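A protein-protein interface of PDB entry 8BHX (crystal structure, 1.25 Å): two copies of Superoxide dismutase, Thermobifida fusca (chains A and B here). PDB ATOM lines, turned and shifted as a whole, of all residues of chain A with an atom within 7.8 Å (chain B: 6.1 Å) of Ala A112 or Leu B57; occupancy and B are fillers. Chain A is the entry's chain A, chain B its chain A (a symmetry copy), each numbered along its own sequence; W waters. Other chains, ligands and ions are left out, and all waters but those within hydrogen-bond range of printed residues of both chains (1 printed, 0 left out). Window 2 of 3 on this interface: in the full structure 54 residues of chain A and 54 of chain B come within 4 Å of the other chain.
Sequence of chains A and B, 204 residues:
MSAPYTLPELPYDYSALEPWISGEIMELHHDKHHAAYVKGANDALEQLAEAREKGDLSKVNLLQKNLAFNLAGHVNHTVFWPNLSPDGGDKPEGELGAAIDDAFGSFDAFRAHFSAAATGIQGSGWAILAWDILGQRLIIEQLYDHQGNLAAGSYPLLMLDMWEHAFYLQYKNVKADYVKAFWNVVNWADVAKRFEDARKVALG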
ATOM      1  N   SER A 106       9.845   6.678   1.294  1.00  0.00           N
ATOM      2  CA  SER A 106      10.618   5.795   0.432  1.00  0.00           C
ATOM      3  C   SER A 106      11.365   4.829   1.342  1.00  0.00           C
ATOM      4  O   SER A 106      11.474   5.046   2.556  1.00  0.00           O
ATOM      5  CB  SER A 106      11.617   6.582  -0.415  1.00  0.00           C
ATOM      6  OG  SER A 106      12.619   7.151   0.419  1.00  0.00           O
ATOM      7  N   PHE A 107      11.895   3.764   0.741  1.00  0.00           N
ATOM      8  CA  PHE A 107      12.739   2.848   1.496  1.00  0.00           C
ATOM      9  C   PHE A 107      13.978   3.562   2.004  1.00  0.00           C
ATOM     10  O   PHE A 107      14.389   3.366   3.155  1.00  0.00           O
ATOM     11  CB  PHE A 107      13.119   1.655   0.626  1.00  0.00           C
ATOM     12  CG  PHE A 107      13.973   0.643   1.324  1.00  0.00           C
ATOM     13  CD1 PHE A 107      15.130   0.171   0.732  1.00  0.00           C
ATOM     14  CD2 PHE A 107      13.613   0.139   2.563  1.00  0.00           C
ATOM     15  CE1 PHE A 107      15.917  -0.781   1.361  1.00  0.00           C
ATOM     16  CE2 PHE A 107      14.402  -0.799   3.210  1.00  0.00           C
ATOM     17  CZ  PHE A 107      15.551  -1.265   2.607  1.00  0.00           C
ATOM     18  N   ASP A 108      14.581   4.411   1.167  1.00  0.00           N
ATOM     19  CA  ASP A 108      15.787   5.117   1.578  1.00  0.00           C
ATOM     20  C   ASP A 108      15.513   6.025   2.773  1.00  0.00           C
ATOM     21  O   ASP A 108      16.335   6.110   3.687  1.00  0.00           O
ATOM     22  CB  ASP A 108      16.344   5.908   0.392  1.00  0.00           C
ATOM     23  CG  ASP A 108      17.179   5.046  -0.550  1.00  0.00           C
ATOM     24  OD1 ASP A 108      17.432   3.864  -0.235  1.00  0.00           O
ATOM     25  OD2 ASP A 108      17.570   5.565  -1.615  1.00  0.00           O
ATOM     26  N   ALA A 109      14.369   6.717   2.780  1.00  0.00           N
ATOM     27  CA  ALA A 109      14.043   7.575   3.919  1.00  0.00           C
ATOM     28  C   ALA A 109      13.761   6.751   5.171  1.00  0.00           C
ATOM     29  O   ALA A 109      14.139   7.145   6.277  1.00  0.00           O
ATOM     30  CB  ALA A 109      12.841   8.458   3.586  1.00  0.00           C
ATOM     31  N   PHE A 110      13.090   5.609   5.014  1.00  0.00           N
ATOM     32  CA  PHE A 110      12.924   4.700   6.134  1.00  0.00           C
ATOM     33  C   PHE A 110      14.280   4.275   6.682  1.00  0.00           C
ATOM     34  O   PHE A 110      14.493   4.275   7.897  1.00  0.00           O
ATOM     35  CB  PHE A 110      12.113   3.471   5.707  1.00  0.00           C
ATOM     36  CG  PHE A 110      12.282   2.323   6.642  1.00  0.00           C
ATOM     37  CD1 PHE A 110      11.638   2.325   7.865  1.00  0.00           C
ATOM     38  CD2 PHE A 110      13.110   1.256   6.331  1.00  0.00           C
ATOM     39  CE1 PHE A 110      11.828   1.295   8.772  1.00  0.00           C
ATOM     40  CE2 PHE A 110      13.287   0.218   7.223  1.00  0.00           C
ATOM     41  CZ  PHE A 110      12.645   0.237   8.447  1.00  0.00           C
ATOM     42  N   ARG A 111      15.207   3.874   5.809  1.00  0.00           N
ATOM     43  CA  ARG A 111      16.517   3.453   6.287  1.00  0.00           C
ATOM     44  C   ARG A 111      17.237   4.577   7.017  1.00  0.00           C
ATOM     45  O   ARG A 111      17.903   4.335   8.026  1.00  0.00           O
ATOM     46  CB  ARG A 111      17.373   2.942   5.125  1.00  0.00           C
ATOM     47  CG  ARG A 111      17.004   1.536   4.646  1.00  0.00           C
ATOM     48  CD  ARG A 111      18.177   0.883   3.952  1.00  0.00           C
ATOM     49  NE  ARG A 111      18.526   1.694   2.794  1.00  0.00           N
ATOM     50  CZ  ARG A 111      19.742   2.147   2.522  1.00  0.00           C
ATOM     51  NH1 ARG A 111      19.925   2.894   1.437  1.00  0.00           N
ATOM     52  NH2 ARG A 111      20.769   1.858   3.320  1.00  0.00           N
ATOM     53  N   ALA A 112      17.139   5.813   6.516  1.00  0.00           N
ATOM     54  CA  ALA A 112      17.811   6.921   7.189  1.00  0.00           C
ATOM     55  C   ALA A 112      17.233   7.132   8.583  1.00  0.00           C
ATOM     56  O   ALA A 112      17.975   7.333   9.547  1.00  0.00           O
ATOM     57  CB  ALA A 112      17.682   8.206   6.370  1.00  0.00           C
ATOM     58  N   HIS A 113      15.904   7.104   8.700  1.00  0.00           N
ATOM     59  CA  HIS A 113      15.258   7.273  10.003  1.00  0.00           C
ATOM     60  C   HIS A 113      15.613   6.122  10.940  1.00  0.00           C
ATOM     61  O   HIS A 113      16.027   6.343  12.081  1.00  0.00           O
ATOM     62  CB  HIS A 113      13.753   7.389   9.727  1.00  0.00           C
ATOM     63  CG  HIS A 113      12.886   7.545  10.929  1.00  0.00           C
ATOM     64  ND1 HIS A 113      11.532   7.765  10.808  1.00  0.00           N
ATOM     65  CD2 HIS A 113      13.153   7.473  12.254  1.00  0.00           C
ATOM     66  CE1 HIS A 113      11.001   7.818  12.013  1.00  0.00           C
ATOM     67  NE2 HIS A 113      11.957   7.645  12.908  1.00  0.00           N
ATOM     68  N   PHE A 114      15.487   4.886  10.454  1.00  0.00           N
ATOM     69  CA  PHE A 114      15.801   3.718  11.270  1.00  0.00           C
ATOM     70  C   PHE A 114      17.259   3.756  11.727  1.00  0.00           C
ATOM     71  O   PHE A 114      17.569   3.491  12.899  1.00  0.00           O
ATOM     72  CB  PHE A 114      15.463   2.463  10.456  1.00  0.00           C
ATOM     73  CG  PHE A 114      15.499   1.171  11.232  1.00  0.00           C
ATOM     74  CD1 PHE A 114      16.684   0.501  11.449  1.00  0.00           C
ATOM     75  CD2 PHE A 114      14.329   0.601  11.700  1.00  0.00           C
ATOM     76  CE1 PHE A 114      16.714  -0.707  12.154  1.00  0.00           C
ATOM     77  CE2 PHE A 114      14.362  -0.611  12.403  1.00  0.00           C
ATOM     78  CZ  PHE A 114      15.560  -1.259  12.613  1.00  0.00           C
ATOM     79  N   SER A 115      18.178   4.093  10.807  1.00  0.00           N
ATOM     80  CA  SER A 115      19.593   4.126  11.154  1.00  0.00           C
ATOM     81  C   SER A 115      19.895   5.211  12.174  1.00  0.00           C
ATOM     82  O   SER A 115      20.709   5.003  13.076  1.00  0.00           O
ATOM     83  CB  SER A 115      20.441   4.342   9.895  1.00  0.00           C
ATOM     84  OG  SER A 115      20.280   3.275   8.956  1.00  0.00           O
ATOM     85  N   ALA A 116      19.245   6.374  12.046  1.00  0.00           N
ATOM     86  CA  ALA A 116      19.431   7.439  13.026  1.00  0.00           C
ATOM     87  C   ALA A 116      18.930   7.009  14.405  1.00  0.00           C
ATOM     88  O   ALA A 116      19.586   7.255  15.427  1.00  0.00           O
ATOM     89  CB  ALA A 116      18.708   8.701  12.564  1.00  0.00           C
ATOM     90  N   ALA A 117      17.771   6.358  14.448  1.00  0.00           N
ATOM     91  CA  ALA A 117      17.265   5.840  15.716  1.00  0.00           C
ATOM     92  C   ALA A 117      18.222   4.812  16.310  1.00  0.00           C
ATOM     93  O   ALA A 117      18.414   4.759  17.536  1.00  0.00           O
ATOM     94  CB  ALA A 117      15.874   5.246  15.498  1.00  0.00           C
ATOM     95  N   ALA A 118      18.844   3.994  15.460  1.00  0.00           N
ATOM     96  CA  ALA A 118      19.738   2.953  15.961  1.00  0.00           C
ATOM     97  C   ALA A 118      21.028   3.544  16.521  1.00  0.00           C
ATOM     98  O   ALA A 118      21.457   3.202  17.628  1.00  0.00           O
ATOM     99  CB  ALA A 118      20.052   1.958  14.842  1.00  0.00           C
ATOM    100  N   THR A 119      21.677   4.435  15.762  1.00  0.00           N
ATOM    101  CA  THR A 119      22.968   4.954  16.197  1.00  0.00           C
ATOM    102  C   THR A 119      22.829   5.984  17.303  1.00  0.00           C
ATOM    103  O   THR A 119      23.789   6.209  18.048  1.00  0.00           O
ATOM    104  CB  THR A 119      23.726   5.547  14.996  1.00  0.00           C
ATOM    105  OG1 THR A 119      23.010   6.653  14.444  1.00  0.00           O
ATOM    106  CG2 THR A 119      23.987   4.490  13.925  1.00  0.00           C
ATOM    107  N   GLY A 120      21.661   6.574  17.456  1.00  0.00           N
ATOM    108  CA  GLY A 120      21.454   7.642  18.410  1.00  0.00           C
ATOM    109  C   GLY A 120      21.262   7.214  19.837  1.00  0.00           C
ATOM    110  O   GLY A 120      21.296   8.070  20.719  1.00  0.00           O
ATOM    111  N   ILE A 140       8.348   3.786  13.688  1.00  0.00           N
ATOM    112  CA  ILE A 140       9.598   3.360  14.297  1.00  0.00           C
ATOM    113  C   ILE A 140       9.500   3.678  15.774  1.00  0.00           C
ATOM    114  O   ILE A 140       8.886   4.682  16.172  1.00  0.00           O
ATOM    115  CB  ILE A 140      10.805   4.046  13.624  1.00  0.00           C
ATOM    116  CG1 ILE A 140      11.039   3.398  12.255  1.00  0.00           C
ATOM    117  CG2 ILE A 140      12.051   3.986  14.490  1.00  0.00           C
ATOM    118  CD1 ILE A 140      12.046   4.122  11.378  1.00  0.00           C
ATOM    119  N   VAL A 179      25.398  -0.885  11.791  1.00  0.00           N
ATOM    120  CA  VAL A 179      24.090  -0.566  11.218  1.00  0.00           C
ATOM    121  C   VAL A 179      24.135  -0.680   9.701  1.00  0.00           C
ATOM    122  O   VAL A 179      23.218  -1.226   9.074  1.00  0.00           O
ATOM    123  CB  VAL A 179      23.624   0.828  11.700  1.00  0.00           C
ATOM    124  CG1 VAL A 179      22.280   1.216  11.064  1.00  0.00           C
ATOM    125  CG2 VAL A 179      23.483   0.867  13.187  1.00  0.00           C
ATOM    126  N   TRP A 183      21.803  -4.004   7.054  1.00  0.00           N
ATOM    127  CA  TRP A 183      20.883  -3.996   5.922  1.00  0.00           C
ATOM    128  C   TRP A 183      21.125  -5.163   4.981  1.00  0.00           C
ATOM    129  O   TRP A 183      20.203  -5.581   4.279  1.00  0.00           O
ATOM    130  CB  TRP A 183      20.951  -2.658   5.185  1.00  0.00           C
ATOM    131  CG  TRP A 183      20.531  -1.545   6.080  1.00  0.00           C
ATOM    132  CD1 TRP A 183      21.330  -0.572   6.605  1.00  0.00           C
ATOM    133  CD2 TRP A 183      19.214  -1.308   6.607  1.00  0.00           C
ATOM    134  NE1 TRP A 183      20.596   0.256   7.413  1.00  0.00           N
ATOM    135  CE2 TRP A 183      19.296  -0.175   7.444  1.00  0.00           C
ATOM    136  CE3 TRP A 183      17.982  -1.950   6.454  1.00  0.00           C
ATOM    137  CZ2 TRP A 183      18.190   0.341   8.115  1.00  0.00           C
ATOM    138  CZ3 TRP A 183      16.881  -1.442   7.130  1.00  0.00           C
ATOM    139  CH2 TRP A 183      16.995  -0.304   7.951  1.00  0.00           C
ATOM    140  N   LEU B  48       8.412  14.111  12.714  1.00  0.00           N
ATOM    141  CA  LEU B  48       9.258  13.067  12.148  1.00  0.00           C
ATOM    142  C   LEU B  48       9.253  13.115  10.628  1.00  0.00           C
ATOM    143  O   LEU B  48      10.297  12.941   9.992  1.00  0.00           O
ATOM    144  CB  LEU B  48       8.814  11.696  12.653  1.00  0.00           C
ATOM    145  CG  LEU B  48       9.308  11.351  14.054  1.00  0.00           C
ATOM    146  CD1 LEU B  48       8.484  10.230  14.657  1.00  0.00           C
ATOM    147  CD2 LEU B  48      10.756  10.970  14.013  1.00  0.00           C
ATOM    148  N   ALA B  51      11.407  15.989   9.666  1.00  0.00           N
ATOM    149  CA  ALA B  51      12.827  15.713   9.863  1.00  0.00           C
ATOM    150  C   ALA B  51      13.367  14.812   8.763  1.00  0.00           C
ATOM    151  O   ALA B  51      14.488  15.021   8.276  1.00  0.00           O
ATOM    152  CB  ALA B  51      13.058  15.090  11.238  1.00  0.00           C
ATOM    153  N   ARG B  52      12.587  13.813   8.341  1.00  0.00           N
ATOM    154  CA  ARG B  52      13.005  12.984   7.220  1.00  0.00           C
ATOM    155  C   ARG B  52      13.177  13.832   5.969  1.00  0.00           C
ATOM    156  O   ARG B  52      14.188  13.727   5.265  1.00  0.00           O
ATOM    157  CB  ARG B  52      11.983  11.878   6.965  1.00  0.00           C
ATOM    158  CG  ARG B  52      12.030  10.731   7.965  1.00  0.00           C
ATOM    159  CD  ARG B  52      11.181   9.526   7.516  1.00  0.00           C
ATOM    160  NE  ARG B  52       9.752   9.844   7.472  1.00  0.00           N
ATOM    161  CZ  ARG B  52       8.899   9.695   8.469  1.00  0.00           C
ATOM    162  NH1 ARG B  52       9.284   9.244   9.657  1.00  0.00           N
ATOM    163  NH2 ARG B  52       7.625  10.049   8.287  1.00  0.00           N
ATOM    164  N   GLY B  55      16.140  16.587   6.358  1.00  0.00           N
ATOM    165  CA  GLY B  55      17.466  16.133   6.731  1.00  0.00           C
ATOM    166  C   GLY B  55      17.861  16.433   8.162  1.00  0.00           C
ATOM    167  O   GLY B  55      19.053  16.622   8.433  1.00  0.00           O
ATOM    168  N   ASP B  56      16.906  16.466   9.091  1.00  0.00           N
ATOM    169  CA  ASP B  56      17.135  16.866  10.476  1.00  0.00           C
ATOM    170  C   ASP B  56      17.003  15.695  11.442  1.00  0.00           C
ATOM    171  O   ASP B  56      16.565  15.862  12.580  1.00  0.00           O
ATOM    172  CB  ASP B  56      16.172  17.984  10.870  1.00  0.00           C
ATOM    173  CG  ASP B  56      16.658  18.796  12.052  1.00  0.00           C
ATOM    174  OD1 ASP B  56      17.870  18.851  12.315  1.00  0.00           O
ATOM    175  OD2 ASP B  56      15.789  19.392  12.722  1.00  0.00           O
ATOM    176  N   LEU B  57      17.424  14.500  11.011  1.00  0.00           N
ATOM    177  CA  LEU B  57      17.306  13.331  11.877  1.00  0.00           C
ATOM    178  C   LEU B  57      18.282  13.347  13.050  1.00  0.00           C
ATOM    179  O   LEU B  57      18.199  12.446  13.902  1.00  0.00           O
ATOM    180  CB  LEU B  57      17.408  12.034  11.081  1.00  0.00           C
ATOM    181  CG  LEU B  57      16.189  11.757  10.200  1.00  0.00           C
ATOM    182  CD1 LEU B  57      16.536  10.673   9.217  1.00  0.00           C
ATOM    183  CD2 LEU B  57      14.984  11.334  10.999  1.00  0.00           C
ATOM    184  N   SER B  58      19.138  14.363  13.178  1.00  0.00           N
ATOM    185  CA  SER B  58      19.881  14.532  14.416  1.00  0.00           C
ATOM    186  C   SER B  58      18.958  14.812  15.592  1.00  0.00           C
ATOM    187  O   SER B  58      19.405  14.707  16.742  1.00  0.00           O
ATOM    188  CB  SER B  58      20.903  15.659  14.297  1.00  0.00           C
ATOM    189  OG  SER B  58      20.250  16.887  14.074  1.00  0.00           O
ATOM    190  N   LYS B  59      17.695  15.141  15.349  1.00  0.00           N
ATOM    191  CA  LYS B  59      16.727  15.317  16.426  1.00  0.00           C
ATOM    192  C   LYS B  59      15.962  14.041  16.751  1.00  0.00           C
ATOM    193  O   LYS B  59      15.029  14.076  17.559  1.00  0.00           O
ATOM    194  CB  LYS B  59      15.766  16.446  16.072  1.00  0.00           C
ATOM    195  CG  LYS B  59      16.455  17.688  15.505  1.00  0.00           C
ATOM    196  CD  LYS B  59      17.632  18.157  16.368  1.00  0.00           C
ATOM    197  CE  LYS B  59      18.182  19.515  15.901  1.00  0.00           C
ATOM    198  NZ  LYS B  59      19.201  19.331  14.824  1.00  0.00           N
ATOM    199  N   VAL B  60      16.387  12.901  16.207  1.00  0.00           N
ATOM    200  CA  VAL B  60      15.603  11.672  16.299  1.00  0.00           C
ATOM    201  C   VAL B  60      15.320  11.255  17.746  1.00  0.00           C
ATOM    202  O   VAL B  60      14.238  10.745  18.042  1.00  0.00           O
ATOM    203  CB  VAL B  60      16.272  10.535  15.498  1.00  0.00           C
ATOM    204  CG1 VAL B  60      17.604  10.154  16.101  1.00  0.00           C
ATOM    205  CG2 VAL B  60      15.320   9.326  15.396  1.00  0.00           C
ATOM    206  N   ASN B  61      16.273  11.440  18.664  1.00  0.00           N
ATOM    207  CA  ASN B  61      16.025  10.979  20.035  1.00  0.00           C
ATOM    208  C   ASN B  61      14.853  11.747  20.639  1.00  0.00           C
ATOM    209  O   ASN B  61      14.016  11.180  21.361  1.00  0.00           O
ATOM    210  CB  ASN B  61      17.257  11.153  20.934  1.00  0.00           C
ATOM    211  CG  ASN B  61      18.425  10.274  20.560  1.00  0.00           C
ATOM    212  OD1 ASN B  61      19.530  10.434  21.107  1.00  0.00           O
ATOM    213  ND2 ASN B  61      18.232   9.392  19.642  1.00  0.00           N
HETATM  214  O   HOH W   1      22.328  10.649  20.099  1.00  0.00           O
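NH1 of Arg B52 is in hydrogen-bond range of ND1 of His A113 (2.9 Å).
The side-chain amide oxygen (OD1) of Asn B61 lies close to the backbone carbonyl oxygen (O) of Gly A120, 3.0 Å away.
N of Ala A109 sits at hydrogen-bond distance from OG of Ser A106, at 3.0 Å.
Among the printed residues, pairs that only touch across the chains: Ala A109 with Arg B52 (3.99 Å), Ala A112 with Leu B57 (3.7 Å), His A113 with Leu B48 (3.7 Å), His A113 with Leu B57 (3.7 Å), Ala A116 with Leu B57 (3.9 Å), Ala A116 with Val B60 (3.6 Å) and Ala A117 with Val B60 (3.96 Å).
Ala A112 touches just one residue of chain B: Leu B57.
Of the printed residues of chain B, Gly A120 touches Asn B61 (3.0 Å).
Leu B57 touches just these residues of chain A: Ala A112, His A113 and Ala A116.
Of the printed residues of chain A, Asn B61 touches Gly A120.
The nearest printed residue of chain B that does not touch Ala A112 is Arg B52 (6.4 Å).
Printed residues of chain B that touch a printed residue of chain A: Leu B48, Arg B52, Leu B57, Val B60 and Asn B61.
Along chain B the printed residues that touch a printed residue of chain A span positions 48 to 61.
Hydrophobic or aromatic side chains of chain A that line the printed part of chain B: Ala A112, His A113 and Ala A116.
Among the printed residues, 9 pairs touch across the chains.
Among the printed residues, no Asp or Glu carboxylate lies within 4 Å of a Lys or Arg side-chain nitrogen of the other chain.
No position is printed for both chains.
Water W1 bridges O of Gly A120 and OD1 of Asn B61.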
